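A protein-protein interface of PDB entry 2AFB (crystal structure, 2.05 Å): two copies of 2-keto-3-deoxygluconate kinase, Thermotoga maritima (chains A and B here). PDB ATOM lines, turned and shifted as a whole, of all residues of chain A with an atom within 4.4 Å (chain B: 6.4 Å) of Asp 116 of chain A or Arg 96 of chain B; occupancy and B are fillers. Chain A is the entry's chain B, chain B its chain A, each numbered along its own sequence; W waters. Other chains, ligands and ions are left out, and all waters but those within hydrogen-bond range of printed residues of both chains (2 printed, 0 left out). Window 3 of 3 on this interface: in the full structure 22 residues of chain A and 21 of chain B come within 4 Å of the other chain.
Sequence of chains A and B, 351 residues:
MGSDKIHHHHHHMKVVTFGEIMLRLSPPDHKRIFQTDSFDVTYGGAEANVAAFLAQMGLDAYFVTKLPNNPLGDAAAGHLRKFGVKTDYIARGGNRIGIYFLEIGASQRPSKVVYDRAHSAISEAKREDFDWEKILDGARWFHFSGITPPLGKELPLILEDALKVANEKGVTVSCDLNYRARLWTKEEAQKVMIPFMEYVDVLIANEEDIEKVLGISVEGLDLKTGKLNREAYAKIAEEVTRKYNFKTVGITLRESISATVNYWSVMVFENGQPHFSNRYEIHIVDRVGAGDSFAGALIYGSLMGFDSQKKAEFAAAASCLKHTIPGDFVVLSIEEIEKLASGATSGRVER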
ATOM      1  N   ARG A  96      24.355   0.206   6.676  1.00  0.00           N
ATOM      2  CA  ARG A  96      24.072  -0.277   5.347  1.00  0.00           C
ATOM      3  C   ARG A  96      22.744   0.138   4.820  1.00  0.00           C
ATOM      4  O   ARG A  96      21.882   0.600   5.550  1.00  0.00           O
ATOM      5  CB  ARG A  96      24.157  -1.811   5.285  1.00  0.00           C
ATOM      6  CG  ARG A  96      23.092  -2.618   6.018  1.00  0.00           C
ATOM      7  CD  ARG A  96      23.349  -4.095   5.624  1.00  0.00           C
ATOM      8  NE  ARG A  96      22.096  -4.672   5.329  1.00  0.00           N
ATOM      9  CZ  ARG A  96      21.641  -5.183   4.200  1.00  0.00           C
ATOM     10  NH1 ARG A  96      22.344  -5.436   3.107  1.00  0.00           N
ATOM     11  NH2 ARG A  96      20.396  -5.539   4.242  1.00  0.00           N
ATOM     12  N   GLY A  98      19.363  -1.232   2.760  1.00  0.00           N
ATOM     13  CA  GLY A  98      18.606  -2.462   2.474  1.00  0.00           C
ATOM     14  C   GLY A  98      18.638  -2.743   0.977  1.00  0.00           C
ATOM     15  O   GLY A  98      18.734  -1.805   0.209  1.00  0.00           O
ATOM     16  N   ILE A  99      18.511  -4.020   0.612  1.00  0.00           N
ATOM     17  CA  ILE A  99      18.599  -4.517  -0.736  1.00  0.00           C
ATOM     18  C   ILE A  99      17.447  -5.475  -0.981  1.00  0.00           C
ATOM     19  O   ILE A  99      17.057  -6.253  -0.100  1.00  0.00           O
ATOM     20  CB  ILE A  99      19.945  -5.324  -0.964  1.00  0.00           C
ATOM     21  CG1 ILE A  99      21.158  -4.439  -0.663  1.00  0.00           C
ATOM     22  CG2 ILE A  99      20.041  -5.883  -2.413  1.00  0.00           C
ATOM     23  CD1 ILE A  99      22.500  -5.115  -0.835  1.00  0.00           C
ATOM     24  N   PHE A 101      16.540  -8.269  -4.317  1.00  0.00           N
ATOM     25  CA  PHE A 101      16.858  -8.832  -5.633  1.00  0.00           C
ATOM     26  C   PHE A 101      15.528  -9.225  -6.248  1.00  0.00           C
ATOM     27  O   PHE A 101      14.701  -9.814  -5.589  1.00  0.00           O
ATOM     28  CB  PHE A 101      17.730 -10.078  -5.507  1.00  0.00           C
ATOM     29  CG  PHE A 101      19.038  -9.843  -4.794  1.00  0.00           C
ATOM     30  CD1 PHE A 101      19.107  -9.862  -3.411  1.00  0.00           C
ATOM     31  CD2 PHE A 101      20.194  -9.635  -5.507  1.00  0.00           C
ATOM     32  CE1 PHE A 101      20.293  -9.643  -2.735  1.00  0.00           C
ATOM     33  CE2 PHE A 101      21.391  -9.403  -4.866  1.00  0.00           C
ATOM     34  CZ  PHE A 101      21.452  -9.396  -3.472  1.00  0.00           C
ATOM     35  N   VAL A 114      14.028 -11.748  -3.509  1.00  0.00           N
ATOM     36  CA  VAL A 114      14.806 -12.140  -2.366  1.00  0.00           C
ATOM     37  C   VAL A 114      15.089 -10.877  -1.577  1.00  0.00           C
ATOM     38  O   VAL A 114      15.751  -9.974  -2.080  1.00  0.00           O
ATOM     39  CB  VAL A 114      16.112 -12.740  -2.831  1.00  0.00           C
ATOM     40  CG1 VAL A 114      16.978 -13.114  -1.614  1.00  0.00           C
ATOM     41  CG2 VAL A 114      15.822 -13.922  -3.749  1.00  0.00           C
ATOM     42  N   TYR A 115      14.603 -10.795  -0.344  1.00  0.00           N
ATOM     43  CA  TYR A 115      14.865  -9.598   0.465  1.00  0.00           C
ATOM     44  C   TYR A 115      16.220  -9.711   1.183  1.00  0.00           C
ATOM     45  O   TYR A 115      16.593 -10.769   1.570  1.00  0.00           O
ATOM     46  CB  TYR A 115      13.740  -9.314   1.457  1.00  0.00           C
ATOM     47  CG  TYR A 115      12.538  -8.712   0.783  1.00  0.00           C
ATOM     48  CD1 TYR A 115      12.548  -7.400   0.376  1.00  0.00           C
ATOM     49  CD2 TYR A 115      11.398  -9.449   0.563  1.00  0.00           C
ATOM     50  CE1 TYR A 115      11.475  -6.842  -0.263  1.00  0.00           C
ATOM     51  CE2 TYR A 115      10.300  -8.886  -0.067  1.00  0.00           C
ATOM     52  CZ  TYR A 115      10.356  -7.591  -0.484  1.00  0.00           C
ATOM     53  OH  TYR A 115       9.281  -7.011  -1.146  1.00  0.00           O
ATOM     54  N   ASP A 116      16.925  -8.590   1.290  1.00  0.00           N
ATOM     55  CA  ASP A 116      18.093  -8.459   2.087  1.00  0.00           C
ATOM     56  C   ASP A 116      18.128  -7.057   2.724  1.00  0.00           C
ATOM     57  O   ASP A 116      19.021  -6.255   2.474  1.00  0.00           O
ATOM     58  CB  ASP A 116      19.306  -8.695   1.221  1.00  0.00           C
ATOM     59  CG  ASP A 116      20.617  -8.787   2.035  1.00  0.00           C
ATOM     60  OD1 ASP A 116      20.567  -9.057   3.273  1.00  0.00           O
ATOM     61  OD2 ASP A 116      21.689  -8.602   1.414  1.00  0.00           O
ATOM     62  N   ARG A 117      17.101  -6.763   3.509  1.00  0.00           N
ATOM     63  CA  ARG A 117      16.896  -5.442   4.118  1.00  0.00           C
ATOM     64  C   ARG A 117      17.167  -5.342   5.627  1.00  0.00           C
ATOM     65  O   ARG A 117      17.174  -4.253   6.169  1.00  0.00           O
ATOM     66  CB  ARG A 117      15.450  -4.986   3.813  1.00  0.00           C
ATOM     67  CG  ARG A 117      14.427  -5.829   4.501  1.00  0.00           C
ATOM     68  CD  ARG A 117      13.006  -5.632   4.009  1.00  0.00           C
ATOM     69  NE  ARG A 117      12.649  -4.232   3.895  1.00  0.00           N
ATOM     70  CZ  ARG A 117      11.611  -3.786   3.187  1.00  0.00           C
ATOM     71  NH1 ARG A 117      10.820  -4.644   2.538  1.00  0.00           N
ATOM     72  NH2 ARG A 117      11.383  -2.476   3.094  1.00  0.00           N
ATOM     73  N   ALA A 118      17.374  -6.458   6.320  1.00  0.00           N
ATOM     74  CA  ALA A 118      17.550  -6.441   7.770  1.00  0.00           C
ATOM     75  C   ALA A 118      18.753  -5.597   8.110  1.00  0.00           C
ATOM     76  O   ALA A 118      19.704  -5.588   7.340  1.00  0.00           O
ATOM     77  CB  ALA A 118      17.748  -7.883   8.361  1.00  0.00           C
ATOM     78  N   GLU B  20      34.744 -17.729   4.022  1.00  0.00           N
ATOM     79  CA  GLU B  20      33.534 -17.073   3.462  1.00  0.00           C
ATOM     80  C   GLU B  20      33.649 -16.752   1.998  1.00  0.00           C
ATOM     81  O   GLU B  20      34.640 -16.169   1.566  1.00  0.00           O
ATOM     82  CB  GLU B  20      33.199 -15.762   4.217  1.00  0.00           C
ATOM     83  CG  GLU B  20      32.014 -15.009   3.620  1.00  0.00           C
ATOM     84  CD  GLU B  20      31.328 -13.992   4.560  1.00  0.00           C
ATOM     85  OE1 GLU B  20      32.014 -13.344   5.372  1.00  0.00           O
ATOM     86  OE2 GLU B  20      30.103 -13.787   4.438  1.00  0.00           O
ATOM     87  N   LYS B  66      29.307 -22.037   4.756  1.00  0.00           N
ATOM     88  CA  LYS B  66      27.859 -22.068   4.906  1.00  0.00           C
ATOM     89  C   LYS B  66      27.303 -20.995   3.976  1.00  0.00           C
ATOM     90  O   LYS B  66      27.847 -19.874   3.886  1.00  0.00           O
ATOM     91  CB  LYS B  66      27.434 -21.818   6.394  1.00  0.00           C
ATOM     92  CG  LYS B  66      26.011 -22.184   6.668  1.00  0.00           C
ATOM     93  CD  LYS B  66      25.606 -21.915   8.076  1.00  0.00           C
ATOM     94  CE  LYS B  66      24.275 -22.627   8.443  1.00  0.00           C
ATOM     95  NZ  LYS B  66      23.891 -22.356   9.897  1.00  0.00           N
ATOM     96  N   LEU B  67      26.261 -21.370   3.235  1.00  0.00           N
ATOM     97  CA  LEU B  67      25.523 -20.448   2.395  1.00  0.00           C
ATOM     98  C   LEU B  67      24.048 -20.589   2.636  1.00  0.00           C
ATOM     99  O   LEU B  67      23.597 -21.682   2.985  1.00  0.00           O
ATOM    100  CB  LEU B  67      25.786 -20.749   0.917  1.00  0.00           C
ATOM    101  CG  LEU B  67      27.228 -20.469   0.497  1.00  0.00           C
ATOM    102  CD1 LEU B  67      27.502 -21.013  -0.861  1.00  0.00           C
ATOM    103  CD2 LEU B  67      27.483 -18.973   0.546  1.00  0.00           C
ATOM    104  N   PRO B  68      23.282 -19.511   2.387  1.00  0.00           N
ATOM    105  CA  PRO B  68      21.845 -19.584   2.600  1.00  0.00           C
ATOM    106  C   PRO B  68      21.223 -20.399   1.495  1.00  0.00           C
ATOM    107  O   PRO B  68      21.748 -20.416   0.415  1.00  0.00           O
ATOM    108  CB  PRO B  68      21.393 -18.127   2.464  1.00  0.00           C
ATOM    109  CG  PRO B  68      22.386 -17.531   1.535  1.00  0.00           C
ATOM    110  CD  PRO B  68      23.688 -18.181   1.892  1.00  0.00           C
ATOM    111  N   ASN B  70      19.083 -19.724  -0.834  1.00  0.00           N
ATOM    112  CA  ASN B  70      18.386 -18.783  -1.652  1.00  0.00           C
ATOM    113  C   ASN B  70      19.175 -18.783  -2.949  1.00  0.00           C
ATOM    114  O   ASN B  70      20.219 -19.404  -3.016  1.00  0.00           O
ATOM    115  CB  ASN B  70      18.220 -17.419  -0.919  1.00  0.00           C
ATOM    116  CG  ASN B  70      19.536 -16.590  -0.787  1.00  0.00           C
ATOM    117  OD1 ASN B  70      20.459 -16.773  -1.552  1.00  0.00           O
ATOM    118  ND2 ASN B  70      19.572 -15.637   0.177  1.00  0.00           N
ATOM    119  N   GLY B  93      21.961 -22.958   5.095  1.00  0.00           N
ATOM    120  CA  GLY B  93      21.176 -22.439   6.188  1.00  0.00           C
ATOM    121  C   GLY B  93      21.493 -20.984   6.399  1.00  0.00           C
ATOM    122  O   GLY B  93      22.275 -20.402   5.674  1.00  0.00           O
ATOM    123  N   GLY B  94      20.870 -20.395   7.407  1.00  0.00           N
ATOM    124  CA  GLY B  94      21.016 -18.966   7.685  1.00  0.00           C
ATOM    125  C   GLY B  94      20.202 -18.089   6.747  1.00  0.00           C
ATOM    126  O   GLY B  94      19.491 -18.588   5.866  1.00  0.00           O
ATOM    127  N   ASN B  95      20.438 -16.784   6.865  1.00  0.00           N
ATOM    128  CA  ASN B  95      19.558 -15.763   6.317  1.00  0.00           C
ATOM    129  C   ASN B  95      19.961 -15.044   5.072  1.00  0.00           C
ATOM    130  O   ASN B  95      19.102 -14.657   4.299  1.00  0.00           O
ATOM    131  CB  ASN B  95      19.262 -14.754   7.430  1.00  0.00           C
ATOM    132  CG  ASN B  95      18.549 -15.400   8.546  1.00  0.00           C
ATOM    133  OD1 ASN B  95      17.602 -16.157   8.312  1.00  0.00           O
ATOM    134  ND2 ASN B  95      19.062 -15.229   9.758  1.00  0.00           N
ATOM    135  N   ARG B  96      21.256 -14.838   4.876  1.00  0.00           N
ATOM    136  CA  ARG B  96      21.757 -14.091   3.739  1.00  0.00           C
ATOM    137  C   ARG B  96      23.170 -14.551   3.389  1.00  0.00           C
ATOM    138  O   ARG B  96      23.874 -15.146   4.219  1.00  0.00           O
ATOM    139  CB  ARG B  96      21.809 -12.582   4.024  1.00  0.00           C
ATOM    140  CG  ARG B  96      22.907 -12.135   5.011  1.00  0.00           C
ATOM    141  CD  ARG B  96      22.703 -10.693   5.463  1.00  0.00           C
ATOM    142  NE  ARG B  96      22.908  -9.741   4.373  1.00  0.00           N
ATOM    143  CZ  ARG B  96      24.091  -9.266   4.007  1.00  0.00           C
ATOM    144  NH1 ARG B  96      25.213  -9.606   4.652  1.00  0.00           N
ATOM    145  NH2 ARG B  96      24.161  -8.428   3.003  1.00  0.00           N
ATOM    146  N   ILE B  97      23.547 -14.255   2.159  1.00  0.00           N
ATOM    147  CA  ILE B  97      24.935 -14.273   1.710  1.00  0.00           C
ATOM    148  C   ILE B  97      25.576 -12.930   1.949  1.00  0.00           C
ATOM    149  O   ILE B  97      24.929 -11.898   1.885  1.00  0.00           O
ATOM    150  CB  ILE B  97      25.076 -14.656   0.236  1.00  0.00           C
ATOM    151  CG1 ILE B  97      26.493 -15.188  -0.050  1.00  0.00           C
ATOM    152  CG2 ILE B  97      24.730 -13.486  -0.702  1.00  0.00           C
ATOM    153  CD1 ILE B  97      26.746 -15.634  -1.519  1.00  0.00           C
ATOM    154  N   GLY B  98      26.841 -12.950   2.311  1.00  0.00           N
ATOM    155  CA  GLY B  98      27.611 -11.729   2.420  1.00  0.00           C
ATOM    156  C   GLY B  98      27.879 -11.155   1.054  1.00  0.00           C
ATOM    157  O   GLY B  98      27.885 -11.878   0.047  1.00  0.00           O
ATOM    158  N   ILE B  99      28.050  -9.837   1.025  1.00  0.00           N
ATOM    159  CA  ILE B  99      28.249  -9.101  -0.192  1.00  0.00           C
ATOM    160  C   ILE B  99      29.393  -8.108  -0.040  1.00  0.00           C
ATOM    161  O   ILE B  99      29.569  -7.515   1.025  1.00  0.00           O
ATOM    162  CB  ILE B  99      26.989  -8.223  -0.555  1.00  0.00           C
ATOM    163  CG1 ILE B  99      25.740  -9.085  -0.633  1.00  0.00           C
ATOM    164  CG2 ILE B  99      27.282  -7.451  -1.820  1.00  0.00           C
ATOM    165  CD1 ILE B  99      24.436  -8.264  -0.868  1.00  0.00           C
ATOM    166  N   ASP B 116      29.405  -5.496   2.912  1.00  0.00           N
ATOM    167  CA  ASP B 116      28.052  -5.762   3.433  1.00  0.00           C
ATOM    168  C   ASP B 116      27.932  -7.259   3.750  1.00  0.00           C
ATOM    169  O   ASP B 116      27.170  -8.000   3.117  1.00  0.00           O
ATOM    170  CB  ASP B 116      27.082  -5.336   2.360  1.00  0.00           C
ATOM    171  CG  ASP B 116      25.644  -5.295   2.840  1.00  0.00           C
ATOM    172  OD1 ASP B 116      25.409  -5.279   4.080  1.00  0.00           O
ATOM    173  OD2 ASP B 116      24.760  -5.315   1.957  1.00  0.00           O
ATOM    174  N   ARG B 117      28.803  -7.707   4.664  1.00  0.00           N
ATOM    175  CA  ARG B 117      29.008  -9.116   4.956  1.00  0.00           C
ATOM    176  C   ARG B 117      28.438  -9.486   6.323  1.00  0.00           C
ATOM    177  O   ARG B 117      28.262 -10.647   6.635  1.00  0.00           O
ATOM    178  CB  ARG B 117      30.505  -9.477   4.827  1.00  0.00           C
ATOM    179  CG  ARG B 117      31.428  -8.814   5.881  1.00  0.00           C
ATOM    180  CD  ARG B 117      32.959  -8.983   5.609  1.00  0.00           C
ATOM    181  NE  ARG B 117      33.265 -10.335   5.183  1.00  0.00           N
ATOM    182  CZ  ARG B 117      34.450 -10.716   4.702  1.00  0.00           C
ATOM    183  NH1 ARG B 117      35.457  -9.827   4.649  1.00  0.00           N
ATOM    184  NH2 ARG B 117      34.614 -11.972   4.269  1.00  0.00           N
ATOM    185  N   ALA B 118      28.079  -8.505   7.120  1.00  0.00           N
ATOM    186  CA  ALA B 118      27.613  -8.805   8.471  1.00  0.00           C
ATOM    187  C   ALA B 118      26.341  -9.637   8.467  1.00  0.00           C
ATOM    188  O   ALA B 118      25.501  -9.507   7.612  1.00  0.00           O
ATOM    189  CB  ALA B 118      27.413  -7.541   9.233  1.00  0.00           C
ATOM    190  N   HIS B 119      26.251 -10.550   9.402  1.00  0.00           N
ATOM    191  CA  HIS B 119      25.063 -11.375   9.611  1.00  0.00           C
ATOM    192  C   HIS B 119      24.855 -12.386   8.495  1.00  0.00           C
ATOM    193  O   HIS B 119      23.776 -12.931   8.364  1.00  0.00           O
ATOM    194  CB  HIS B 119      23.803 -10.507   9.810  1.00  0.00           C
ATOM    195  CG  HIS B 119      23.991  -9.385  10.774  1.00  0.00           C
ATOM    196  ND1 HIS B 119      24.164  -9.585  12.128  1.00  0.00           N
ATOM    197  CD2 HIS B 119      24.020  -8.042  10.582  1.00  0.00           C
ATOM    198  CE1 HIS B 119      24.308  -8.413  12.727  1.00  0.00           C
ATOM    199  NE2 HIS B 119      24.215  -7.461  11.812  1.00  0.00           N
ATOM    200  N   SER B 120      25.911 -12.646   7.730  1.00  0.00           N
ATOM    201  CA  SER B 120      25.917 -13.693   6.726  1.00  0.00           C
ATOM    202  C   SER B 120      25.776 -15.050   7.387  1.00  0.00           C
ATOM    203  O   SER B 120      26.105 -15.223   8.575  1.00  0.00           O
ATOM    204  CB  SER B 120      27.244 -13.685   5.920  1.00  0.00           C
ATOM    205  OG  SER B 120      28.360 -14.041   6.759  1.00  0.00           O
ATOM    206  N   ALA B 121      25.323 -16.025   6.591  1.00  0.00           N
ATOM    207  CA  ALA B 121      25.103 -17.370   7.075  1.00  0.00           C
ATOM    208  C   ALA B 121      26.400 -17.963   7.696  1.00  0.00           C
ATOM    209  O   ALA B 121      26.361 -18.626   8.721  1.00  0.00           O
ATOM    210  CB  ALA B 121      24.570 -18.247   5.917  1.00  0.00           C
ATOM    211  N   ILE B 122      27.546 -17.724   7.077  1.00  0.00           N
ATOM    212  CA  ILE B 122      28.794 -18.261   7.630  1.00  0.00           C
ATOM    213  C   ILE B 122      29.152 -17.552   8.934  1.00  0.00           C
ATOM    214  O   ILE B 122      29.638 -18.196   9.863  1.00  0.00           O
ATOM    215  CB  ILE B 122      29.978 -18.232   6.594  1.00  0.00           C
ATOM    216  CG1 ILE B 122      31.283 -18.797   7.169  1.00  0.00           C
ATOM    217  CG2 ILE B 122      30.279 -16.817   6.100  1.00  0.00           C
ATOM    218  CD1 ILE B 122      31.266 -20.258   7.358  1.00  0.00           C
HETATM  219  O   HOH W   1      18.875 -12.526   2.020  1.00  0.00           O
HETATM  220  O   HOH W   2      22.552 -10.942   0.389  1.00  0.00           O
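Of the printed residues of chain B, Arg 96 of chain A touches Arg 96 (3.5 Å) and Asp 116 (2.7 Å).
Printed residues of chain B within 4 Å of Ile 99 of chain A: Ile 99 (3.7 Å) and Asp 116 (3.6 Å).
Asp 116 of chain A touches just these residues of chain B: Arg 96 and Ile 99.
Arg 96 of chain B touches just these residues of chain A: Arg 96 (3.5 Å) and Asp 116 (2.7 Å).
Of the printed residues of chain A, Ile 99 of chain B touches Ile 99 (3.7 Å) and Asp 116 (3.6 Å).
Printed residues of chain A within 4 Å of Asp 116 of chain B: Arg 96 (2.7 Å) and Ile 99 (3.6 Å).
The nearest printed residue of chain A that does not touch Ile 99 of chain B is Phe 101 of chain A (4.1 Å).
Of the 19 printed residues of chain B, 3 touch a printed residue of chain A.
Hydrophobic or aromatic side chains of chain B within 4 Å of the printed part of chain A: Ile 99.
Of the 9 printed residues of chain A, 3 touch a printed residue of chain B.
Among the printed residues, Asp or Glu carboxylates within 4 Å of a Lys or Arg side-chain nitrogen of the other chain: Arg 96 of chain A with Asp 116 of chain B and Asp 116 of chain A with Arg 96 of chain B.
The guanidinium group of Arg 96 of chain B lies within salt-bridge range of the side-chain carboxylate of Asp 116 of chain A, 2.7 Å away.
The guanidinium group (NH1) of Arg 96 of chain A lies within salt-bridge range of the side-chain carboxylate (OD2) of Asp 116 of chain B, 2.7 Å away.
The guanidinium group (NH2) of Arg 96 of chain B is in salt-bridge range of the side-chain carboxylate (OD2) of Asp 116 of chain B, at 3.3 Å.
O of Arg 96 of chain B lies within hydrogen-bond range of N of Ala 121 of chain B, at 2.9 Å.
O of Ile 99 of chain B lies within hydrogen-bond range of N of Asp 116 of chain B, at 2.8 Å.
The guanidinium group of Arg 96 of chain A is in salt-bridge range of the side-chain carboxylate of Asp 116 of chain A (3.6 Å).
NH2 of Arg 96 of chain A is in hydrogen-bond range of O of Ala 118 of chain A.
O of Ile 99 of chain A lies within hydrogen-bond range of N of Asp 116 of chain A.
Arg 96 of chain A touches Arg 96 of chain B (NH1 to NH2, 3.5 Å).
Ile 99 of chain B touches Ile 99 of chain A.
CD1 of Ile 99 of chain A touches OD2 of Asp 116 of chain B (3.6 Å).
Ile 99 of chain B touches Asp 116 of chain A.
Arg 96 of chain A touches its own counterpart, Arg 96 of chain B.
Arg 96 of chain A touches Asp 116 of chain B, and with the chains exchanged Asp 116 of chain A touches Arg 96 of chain B.
Ile 99 of chain B touches its own counterpart, Ile 99 of chain A.
Ile 99 of chain A touches Asp 116 of chain B, and with the chains exchanged Asp 116 of chain A touches Ile 99 of chain B.
Positions printed for both chains: 96, 98, 99, 116, 117 and 118.
Of the 6 pairs that touch across the chains among the printed residues, 6 have their exchanged pair printed and touching as well.
Water W2 lies within hydrogen-bond range of the side-chain carboxylate (OD2) of Asp 116 of chain A (2.7 Å) and the backbone carbonyl oxygen (O) of Ile 97 of chain B (3.0 Å).
Water W1 bridges the backbone carbonyl oxygen of Tyr 115 of chain A (2.9 Å) and the backbone carbonyl oxygen of Asn 95 of chain B (3.1 Å).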
